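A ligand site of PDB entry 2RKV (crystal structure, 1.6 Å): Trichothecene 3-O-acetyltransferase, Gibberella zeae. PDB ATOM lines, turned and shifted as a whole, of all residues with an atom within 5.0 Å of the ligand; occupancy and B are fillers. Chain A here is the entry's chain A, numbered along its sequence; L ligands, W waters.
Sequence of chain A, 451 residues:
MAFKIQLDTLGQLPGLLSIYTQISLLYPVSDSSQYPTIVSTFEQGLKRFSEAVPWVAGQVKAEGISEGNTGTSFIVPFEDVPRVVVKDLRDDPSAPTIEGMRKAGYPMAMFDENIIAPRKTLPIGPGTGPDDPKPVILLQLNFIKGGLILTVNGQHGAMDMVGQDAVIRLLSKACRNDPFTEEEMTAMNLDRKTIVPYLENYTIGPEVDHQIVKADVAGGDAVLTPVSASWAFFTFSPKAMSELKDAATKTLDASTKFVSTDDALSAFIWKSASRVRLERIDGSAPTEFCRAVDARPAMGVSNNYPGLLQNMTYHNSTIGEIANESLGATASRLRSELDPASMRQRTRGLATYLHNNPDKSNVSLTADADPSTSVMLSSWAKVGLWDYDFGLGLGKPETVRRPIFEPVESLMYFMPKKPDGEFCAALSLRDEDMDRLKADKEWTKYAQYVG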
ATOM      1  N   GLY A  15       2.921  -2.962 -17.362  1.00  0.00           N
ATOM      2  CA  GLY A  15       4.042  -2.294 -16.692  1.00  0.00           C
ATOM      3  C   GLY A  15       3.584  -1.237 -15.708  1.00  0.00           C
ATOM      4  O   GLY A  15       4.122  -1.158 -14.596  1.00  0.00           O
ATOM      5  N   LEU A  16       2.596  -0.442 -16.107  1.00  0.00           N
ATOM      6  CA  LEU A  16       2.111   0.655 -15.274  1.00  0.00           C
ATOM      7  C   LEU A  16       1.356   0.153 -14.055  1.00  0.00           C
ATOM      8  O   LEU A  16       1.413   0.762 -12.982  1.00  0.00           O
ATOM      9  CB  LEU A  16       1.240   1.590 -16.101  1.00  0.00           C
ATOM     10  CG  LEU A  16       1.933   2.275 -17.283  1.00  0.00           C
ATOM     11  CD1 LEU A  16       1.001   3.287 -17.913  1.00  0.00           C
ATOM     12  CD2 LEU A  16       3.237   2.941 -16.859  1.00  0.00           C
ATOM     13  N   ILE A  19       3.689  -0.535 -10.843  1.00  0.00           N
ATOM     14  CA  ILE A  19       4.651   0.505 -10.492  1.00  0.00           C
ATOM     15  C   ILE A  19       3.994   1.625  -9.671  1.00  0.00           C
ATOM     16  O   ILE A  19       2.837   1.971  -9.914  1.00  0.00           O
ATOM     17  CB  ILE A  19       5.276   1.130 -11.769  1.00  0.00           C
ATOM     18  CG1 ILE A  19       6.218   0.117 -12.454  1.00  0.00           C
ATOM     19  CG2 ILE A  19       6.021   2.429 -11.460  1.00  0.00           C
ATOM     20  CD1 ILE A  19       6.679   0.579 -13.843  1.00  0.00           C
ATOM     21  N   THR A  21       4.851   5.683  -8.823  1.00  0.00           N
ATOM     22  CA  THR A  21       5.661   6.882  -9.048  1.00  0.00           C
ATOM     23  C   THR A  21       5.829   7.627  -7.731  1.00  0.00           C
ATOM     24  O   THR A  21       4.841   7.973  -7.087  1.00  0.00           O
ATOM     25  CB  THR A  21       4.992   7.833 -10.054  1.00  0.00           C
ATOM     26  OG1 THR A  21       4.764   7.140 -11.294  1.00  0.00           O
ATOM     27  CG2 THR A  21       5.872   9.067 -10.304  1.00  0.00           C
ATOM     28  N   THR A 121       8.995   1.716  -5.448  1.00  0.00           N
ATOM     29  CA  THR A 121       8.634   1.981  -6.841  1.00  0.00           C
ATOM     30  C   THR A 121       8.258   0.703  -7.592  1.00  0.00           C
ATOM     31  O   THR A 121       7.241   0.650  -8.296  1.00  0.00           O
ATOM     32  CB  THR A 121       9.797   2.673  -7.565  1.00  0.00           C
ATOM     33  OG1 THR A 121      10.013   3.961  -6.991  1.00  0.00           O
ATOM     34  CG2 THR A 121       9.498   2.804  -9.051  1.00  0.00           C
ATOM     35  N   LEU A 122       9.094  -0.329  -7.433  1.00  0.00           N
ATOM     36  CA  LEU A 122       8.924  -1.572  -8.151  1.00  0.00           C
ATOM     37  C   LEU A 122       8.248  -2.624  -7.279  1.00  0.00           C
ATOM     38  O   LEU A 122       8.304  -2.521  -6.055  1.00  0.00           O
ATOM     39  CB  LEU A 122      10.290  -2.067  -8.665  1.00  0.00           C
ATOM     40  CG  LEU A 122      11.035  -1.084  -9.574  1.00  0.00           C
ATOM     41  CD1 LEU A 122      12.466  -1.557  -9.888  1.00  0.00           C
ATOM     42  CD2 LEU A 122      10.257  -0.782 -10.878  1.00  0.00           C
ATOM     43  N   HIS A 156       0.716   3.855 -10.761  1.00  0.00           N
ATOM     44  CA  HIS A 156       0.887   4.338 -12.121  1.00  0.00           C
ATOM     45  C   HIS A 156      -0.208   3.990 -13.125  1.00  0.00           C
ATOM     46  O   HIS A 156      -0.308   4.646 -14.085  1.00  0.00           O
ATOM     47  CB  HIS A 156       2.276   3.927 -12.697  1.00  0.00           C
ATOM     48  CG  HIS A 156       2.864   4.883 -13.699  1.00  0.00           C
ATOM     49  ND1 HIS A 156       2.138   5.569 -14.634  1.00  0.00           N
ATOM     50  CD2 HIS A 156       4.129   5.270 -13.888  1.00  0.00           C
ATOM     51  CE1 HIS A 156       2.932   6.324 -15.371  1.00  0.00           C
ATOM     52  NE2 HIS A 156       4.163   6.146 -14.940  1.00  0.00           N
ATOM     53  N   ALA A 292       8.771  10.251 -22.944  1.00  0.00           N
ATOM     54  CA  ALA A 292       7.410  10.338 -22.409  1.00  0.00           C
ATOM     55  C   ALA A 292       6.770  11.658 -22.808  1.00  0.00           C
ATOM     56  O   ALA A 292       7.389  12.727 -22.703  1.00  0.00           O
ATOM     57  CB  ALA A 292       7.400  10.172 -20.897  1.00  0.00           C
ATOM     58  N   LEU A 308      -4.235   8.646 -16.280  1.00  0.00           N
ATOM     59  CA  LEU A 308      -3.076   8.220 -17.039  1.00  0.00           C
ATOM     60  C   LEU A 308      -3.378   8.473 -18.513  1.00  0.00           C
ATOM     61  O   LEU A 308      -4.193   7.781 -19.131  1.00  0.00           O
ATOM     62  CB  LEU A 308      -2.767   6.742 -16.753  1.00  0.00           C
ATOM     63  CG  LEU A 308      -1.521   6.035 -17.312  1.00  0.00           C
ATOM     64  CD1 LEU A 308      -1.566   5.901 -18.841  1.00  0.00           C
ATOM     65  CD2 LEU A 308      -0.267   6.731 -16.892  1.00  0.00           C
ATOM     66  N   GLN A 310      -0.817   9.349 -21.358  1.00  0.00           N
ATOM     67  CA  GLN A 310       0.546   9.574 -21.755  1.00  0.00           C
ATOM     68  C   GLN A 310       0.893   8.591 -22.859  1.00  0.00           C
ATOM     69  O   GLN A 310       0.307   7.508 -22.967  1.00  0.00           O
ATOM     70  CB  GLN A 310       1.484   9.365 -20.548  1.00  0.00           C
ATOM     71  CG  GLN A 310       2.907   9.741 -20.846  1.00  0.00           C
ATOM     72  CD  GLN A 310       3.637  10.314 -19.663  1.00  0.00           C
ATOM     73  OE1 GLN A 310       3.704   9.728 -18.581  1.00  0.00           O
ATOM     74  NE2 GLN A 310       4.194  11.490 -19.873  1.00  0.00           N
ATOM     75  N   ASN A 311       1.817   9.011 -23.714  1.00  0.00           N
ATOM     76  CA  ASN A 311       2.393   8.102 -24.680  1.00  0.00           C
ATOM     77  C   ASN A 311       3.889   8.341 -24.694  1.00  0.00           C
ATOM     78  O   ASN A 311       4.422   9.064 -23.835  1.00  0.00           O
ATOM     79  CB  ASN A 311       1.758   8.350 -26.055  1.00  0.00           C
ATOM     80  CG  ASN A 311       1.783   7.111 -26.950  1.00  0.00           C
ATOM     81  OD1 ASN A 311       2.552   6.170 -26.715  1.00  0.00           O
ATOM     82  ND2 ASN A 311       0.918   7.099 -27.959  1.00  0.00           N
ATOM     83  N   MET A 312       4.590   7.707 -25.632  1.00  0.00           N
ATOM     84  CA  MET A 312       6.004   7.970 -25.888  1.00  0.00           C
ATOM     85  C   MET A 312       6.156   8.414 -27.334  1.00  0.00           C
ATOM     86  O   MET A 312       5.311   8.106 -28.181  1.00  0.00           O
ATOM     87  CB  MET A 312       6.833   6.691 -25.708  1.00  0.00           C
ATOM     88  CG  MET A 312       6.586   5.913 -24.414  1.00  0.00           C
ATOM     89  SD  MET A 312       7.153   6.781 -22.941  1.00  0.00           S
ATOM     90  CE  MET A 312       8.921   6.712 -23.172  1.00  0.00           C
ATOM     91  N   SER A 364       4.007  -2.880 -24.347  1.00  0.00           N
ATOM     92  CA  SER A 364       4.952  -2.191 -23.486  1.00  0.00           C
ATOM     93  C   SER A 364       5.400  -0.914 -24.163  1.00  0.00           C
ATOM     94  O   SER A 364       5.723  -0.914 -25.359  1.00  0.00           O
ATOM     95  CB  SER A 364       6.166  -3.064 -23.191  1.00  0.00           C
ATOM     96  OG  SER A 364       7.140  -2.334 -22.461  1.00  0.00           O
ATOM     97  N   LEU A 365       5.422   0.176 -23.407  1.00  0.00           N
ATOM     98  CA  LEU A 365       5.924   1.461 -23.900  1.00  0.00           C
ATOM     99  C   LEU A 365       7.401   1.406 -24.275  1.00  0.00           C
ATOM    100  O   LEU A 365       7.905   2.305 -24.962  1.00  0.00           O
ATOM    101  CB  LEU A 365       5.674   2.566 -22.863  1.00  0.00           C
ATOM    102  CG  LEU A 365       4.197   2.903 -22.613  1.00  0.00           C
ATOM    103  CD1 LEU A 365       4.039   3.629 -21.288  1.00  0.00           C
ATOM    104  CD2 LEU A 365       3.611   3.712 -23.775  1.00  0.00           C
ATOM    105  N   THR A 366       8.108   0.379 -23.808  1.00  0.00           N
ATOM    106  CA  THR A 366       9.521   0.219 -24.144  1.00  0.00           C
ATOM    107  C   THR A 366       9.801  -1.149 -24.767  1.00  0.00           C
ATOM    108  O   THR A 366      10.870  -1.739 -24.541  1.00  0.00           O
ATOM    109  CB  THR A 366      10.447   0.427 -22.926  1.00  0.00           C
ATOM    110  OG1 THR A 366      10.078  -0.501 -21.894  1.00  0.00           O
ATOM    111  CG2 THR A 366      10.360   1.872 -22.413  1.00  0.00           C
ATOM    112  N   MET A 376      15.512   6.085 -22.081  1.00  0.00           N
ATOM    113  CA  MET A 376      14.080   6.118 -21.763  1.00  0.00           C
ATOM    114  C   MET A 376      13.873   7.259 -20.788  1.00  0.00           C
ATOM    115  O   MET A 376      14.188   7.130 -19.601  1.00  0.00           O
ATOM    116  CB  MET A 376      13.619   4.795 -21.152  1.00  0.00           C
ATOM    117  CG  MET A 376      13.930   3.557 -22.015  1.00  0.00           C
ATOM    118  SD  MET A 376      13.722   1.981 -21.164  1.00  0.00           S
ATOM    119  CE  MET A 376      15.040   2.058 -19.943  1.00  0.00           C
ATOM    120  N   LEU A 377      13.379   8.392 -21.279  1.00  0.00           N
ATOM    121  CA  LEU A 377      13.324   9.631 -20.491  1.00  0.00           C
ATOM    122  C   LEU A 377      11.904  10.123 -20.262  1.00  0.00           C
ATOM    123  O   LEU A 377      11.091  10.176 -21.204  1.00  0.00           O
ATOM    124  CB  LEU A 377      14.140  10.742 -21.158  1.00  0.00           C
ATOM    125  CG  LEU A 377      13.887  12.163 -20.614  1.00  0.00           C
ATOM    126  CD1 LEU A 377      14.579  12.367 -19.264  1.00  0.00           C
ATOM    127  CD2 LEU A 377      14.310  13.227 -21.595  1.00  0.00           C
ATOM    128  N   SER A 378      11.598  10.487 -19.016  1.00  0.00           N
ATOM    129  CA  SER A 378      10.353  11.173 -18.700  1.00  0.00           C
ATOM    130  C   SER A 378      10.620  12.507 -18.026  1.00  0.00           C
ATOM    131  O   SER A 378      11.201  12.554 -16.940  1.00  0.00           O
ATOM    132  CB  SER A 378       9.427  10.324 -17.831  1.00  0.00           C
ATOM    133  OG  SER A 378       8.211  11.014 -17.572  1.00  0.00           O
ATOM    134  N   PHE A 405      15.846   4.416  -6.250  1.00  0.00           N
ATOM    135  CA  PHE A 405      15.400   3.034  -6.166  1.00  0.00           C
ATOM    136  C   PHE A 405      16.403   2.164  -6.924  1.00  0.00           C
ATOM    137  O   PHE A 405      17.539   2.613  -7.177  1.00  0.00           O
ATOM    138  CB  PHE A 405      13.942   2.865  -6.642  1.00  0.00           C
ATOM    139  CG  PHE A 405      13.682   3.252  -8.083  1.00  0.00           C
ATOM    140  CD1 PHE A 405      13.340   2.280  -9.027  1.00  0.00           C
ATOM    141  CD2 PHE A 405      13.690   4.588  -8.494  1.00  0.00           C
ATOM    142  CE1 PHE A 405      13.069   2.618 -10.360  1.00  0.00           C
ATOM    143  CE2 PHE A 405      13.414   4.945  -9.828  1.00  0.00           C
ATOM    144  CZ  PHE A 405      13.102   3.939 -10.764  1.00  0.00           C
ATOM    145  N   VAL A 408      17.915   1.154 -13.074  1.00  0.00           N
ATOM    146  CA  VAL A 408      17.246   0.645 -14.251  1.00  0.00           C
ATOM    147  C   VAL A 408      17.983   1.267 -15.436  1.00  0.00           C
ATOM    148  O   VAL A 408      17.795   2.453 -15.730  1.00  0.00           O
ATOM    149  CB  VAL A 408      15.747   1.068 -14.298  1.00  0.00           C
ATOM    150  CG1 VAL A 408      15.072   0.554 -15.566  1.00  0.00           C
ATOM    151  CG2 VAL A 408      15.007   0.571 -13.052  1.00  0.00           C
ATOM    152  N   LEU A 411      17.127   4.411 -17.925  1.00  0.00           N
ATOM    153  CA  LEU A 411      15.971   5.165 -17.447  1.00  0.00           C
ATOM    154  C   LEU A 411      16.407   6.538 -16.938  1.00  0.00           C
ATOM    155  O   LEU A 411      17.422   6.652 -16.227  1.00  0.00           O
ATOM    156  CB  LEU A 411      15.253   4.390 -16.335  1.00  0.00           C
ATOM    157  CG  LEU A 411      13.946   4.981 -15.787  1.00  0.00           C
ATOM    158  CD1 LEU A 411      12.899   5.161 -16.892  1.00  0.00           C
ATOM    159  CD2 LEU A 411      13.423   4.064 -14.678  1.00  0.00           C
ATOM    160  N   TYR A 413      14.954  10.759 -15.712  1.00  0.00           N
ATOM    161  CA  TYR A 413      13.913  11.745 -15.414  1.00  0.00           C
ATOM    162  C   TYR A 413      14.460  13.173 -15.407  1.00  0.00           C
ATOM    163  O   TYR A 413      15.631  13.388 -15.078  1.00  0.00           O
ATOM    164  CB  TYR A 413      13.274  11.479 -14.040  1.00  0.00           C
ATOM    165  CG  TYR A 413      12.629  10.127 -13.934  1.00  0.00           C
ATOM    166  CD1 TYR A 413      13.318   9.037 -13.409  1.00  0.00           C
ATOM    167  CD2 TYR A 413      11.317   9.929 -14.383  1.00  0.00           C
ATOM    168  CE1 TYR A 413      12.721   7.775 -13.339  1.00  0.00           C
ATOM    169  CE2 TYR A 413      10.718   8.677 -14.313  1.00  0.00           C
ATOM    170  CZ  TYR A 413      11.416   7.600 -13.780  1.00  0.00           C
ATOM    171  OH  TYR A 413      10.813   6.357 -13.721  1.00  0.00           O
HETATM  172  O1  LIG L   1      11.231   0.796 -16.983  1.00  0.00           O
HETATM  173  C1  LIG L   1      10.300   0.498 -16.360  1.00  0.00           C
HETATM  174  C2  LIG L   1       9.816  -0.895 -16.106  1.00  0.00           C
HETATM  175  C3  LIG L   1      10.122  -1.327 -14.751  1.00  0.00           C
HETATM  176  C4  LIG L   1      11.541  -1.289 -14.513  1.00  0.00           C
HETATM  177  C5  LIG L   1       9.789  -2.746 -14.389  1.00  0.00           C
HETATM  178  O2  LIG L   1       9.540   1.414 -15.750  1.00  0.00           O
HETATM  179  C6  LIG L   1       9.952   2.795 -15.685  1.00  0.00           C
HETATM  180  C7  LIG L   1       9.562   3.552 -16.908  1.00  0.00           C
HETATM  181  C8  LIG L   1       9.390   3.310 -14.416  1.00  0.00           C
HETATM  182  C9  LIG L   1       9.913   2.623 -13.181  1.00  0.00           C
HETATM  183  C10 LIG L   1       8.504   4.246 -14.396  1.00  0.00           C
HETATM  184  C11 LIG L   1       7.965   4.930 -15.608  1.00  0.00           C
HETATM  185  O3  LIG L   1       8.714   6.153 -15.691  1.00  0.00           O
HETATM  186  C12 LIG L   1       8.144   4.127 -16.910  1.00  0.00           C
HETATM  187  C13 LIG L   1       7.130   2.998 -16.920  1.00  0.00           C
HETATM  188  O4  LIG L   1       7.609   1.912 -17.713  1.00  0.00           O
HETATM  189  C14 LIG L   1       6.801   1.205 -18.474  1.00  0.00           C
HETATM  190  C15 LIG L   1       7.562   0.102 -19.172  1.00  0.00           C
HETATM  191  O5  LIG L   1       5.688   1.369 -18.629  1.00  0.00           O
HETATM  192  C16 LIG L   1       7.895   5.099 -18.144  1.00  0.00           C
HETATM  193  C17 LIG L   1       7.886   4.386 -19.512  1.00  0.00           C
HETATM  194  C18 LIG L   1       8.941   6.208 -18.046  1.00  0.00           C
HETATM  195  C19 LIG L   1       8.501   6.941 -16.826  1.00  0.00           C
HETATM  196  C20 LIG L   1      10.161   6.369 -18.770  1.00  0.00           C
HETATM  197  O6  LIG L   1       9.003   7.033 -19.221  1.00  0.00           O
HETATM  198  C21 LIG L   1       6.603   5.947 -17.894  1.00  0.00           C
HETATM  199  C22 LIG L   1       7.051   7.160 -17.110  1.00  0.00           C
HETATM  200  O7  LIG L   1       6.305   7.364 -15.947  1.00  0.00           O
HETATM  201  O8  LIG L   1       6.180   6.397 -19.189  1.00  0.00           O
HETATM  202  C23 LIG L   1       4.946   6.700 -19.558  1.00  0.00           C
HETATM  203  O9  LIG L   1       4.673   7.068 -20.649  1.00  0.00           O
HETATM  204  C24 LIG L   1       4.027   6.588 -18.453  1.00  0.00           C
HETATM  205  O   HOH W   1       4.341  -0.017 -20.669  1.00  0.00           O
HETATM  206  O   HOH W   2       7.026   7.153 -12.880  1.00  0.00           O
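The backbone carbonyl oxygen of Ile 19 lies within hydrogen-bond range of the backbone NH of His 156, at 3.0 Å.
The backbone NH of Thr 366 sits close to the side-chain hydroxyl of Ser 364 (3.2 Å).
The backbone NH (N) of Ala 292 sits at hydrogen-bond distance from the backbone carbonyl oxygen (O) of Leu 377 (2.9 Å).
Water W1 lies within hydrogen-bond range of O5 of the ligand (2.8 Å) and N of Leu 365 (2.9 Å).
Water W2 bridges the side-chain hydroxyl of Thr 21 (2.8 Å) and an oxygen (O7) of the ligand (3.2 Å).
O9 of the ligand lies close to SD of Met 312 (3.4 Å).
Leu 16 touches the ligand.
Ile 19 touches the ligand.
Leu 122 touches the ligand (CD2 to C4, 3.9 Å).
Ala 292 touches the ligand.
OE1 of Gln 310 touches C24 of the ligand, at 3.2 Å.
Asn 311 touches the ligand.
Leu 365 touches the ligand.
OG1 of Thr 366 touches C15 of the ligand, 3.8 Å away.
Ser 378 touches the ligand.
Leu 411 touches the ligand.
Hydrophobic or aromatic side chains within 4 Å of the ligand: Leu 16, Ile 19, Leu 122, His 156, Ala 292, Met 312, Leu 365, Leu 411 and Tyr 413.
Of the 22 residues printed, 13 come within 4 Å of the ligand.
The nearest printed residue that does not touch the ligand is Val 408 (4.1 Å).
O7 of the ligand is in hydrogen-bond range of NE2 of His 156 (2.7 Å).
The side-chain hydroxyl (OH) of Tyr 413 is in hydrogen-bond range of an oxygen (O3) of the ligand (2.9 Å).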
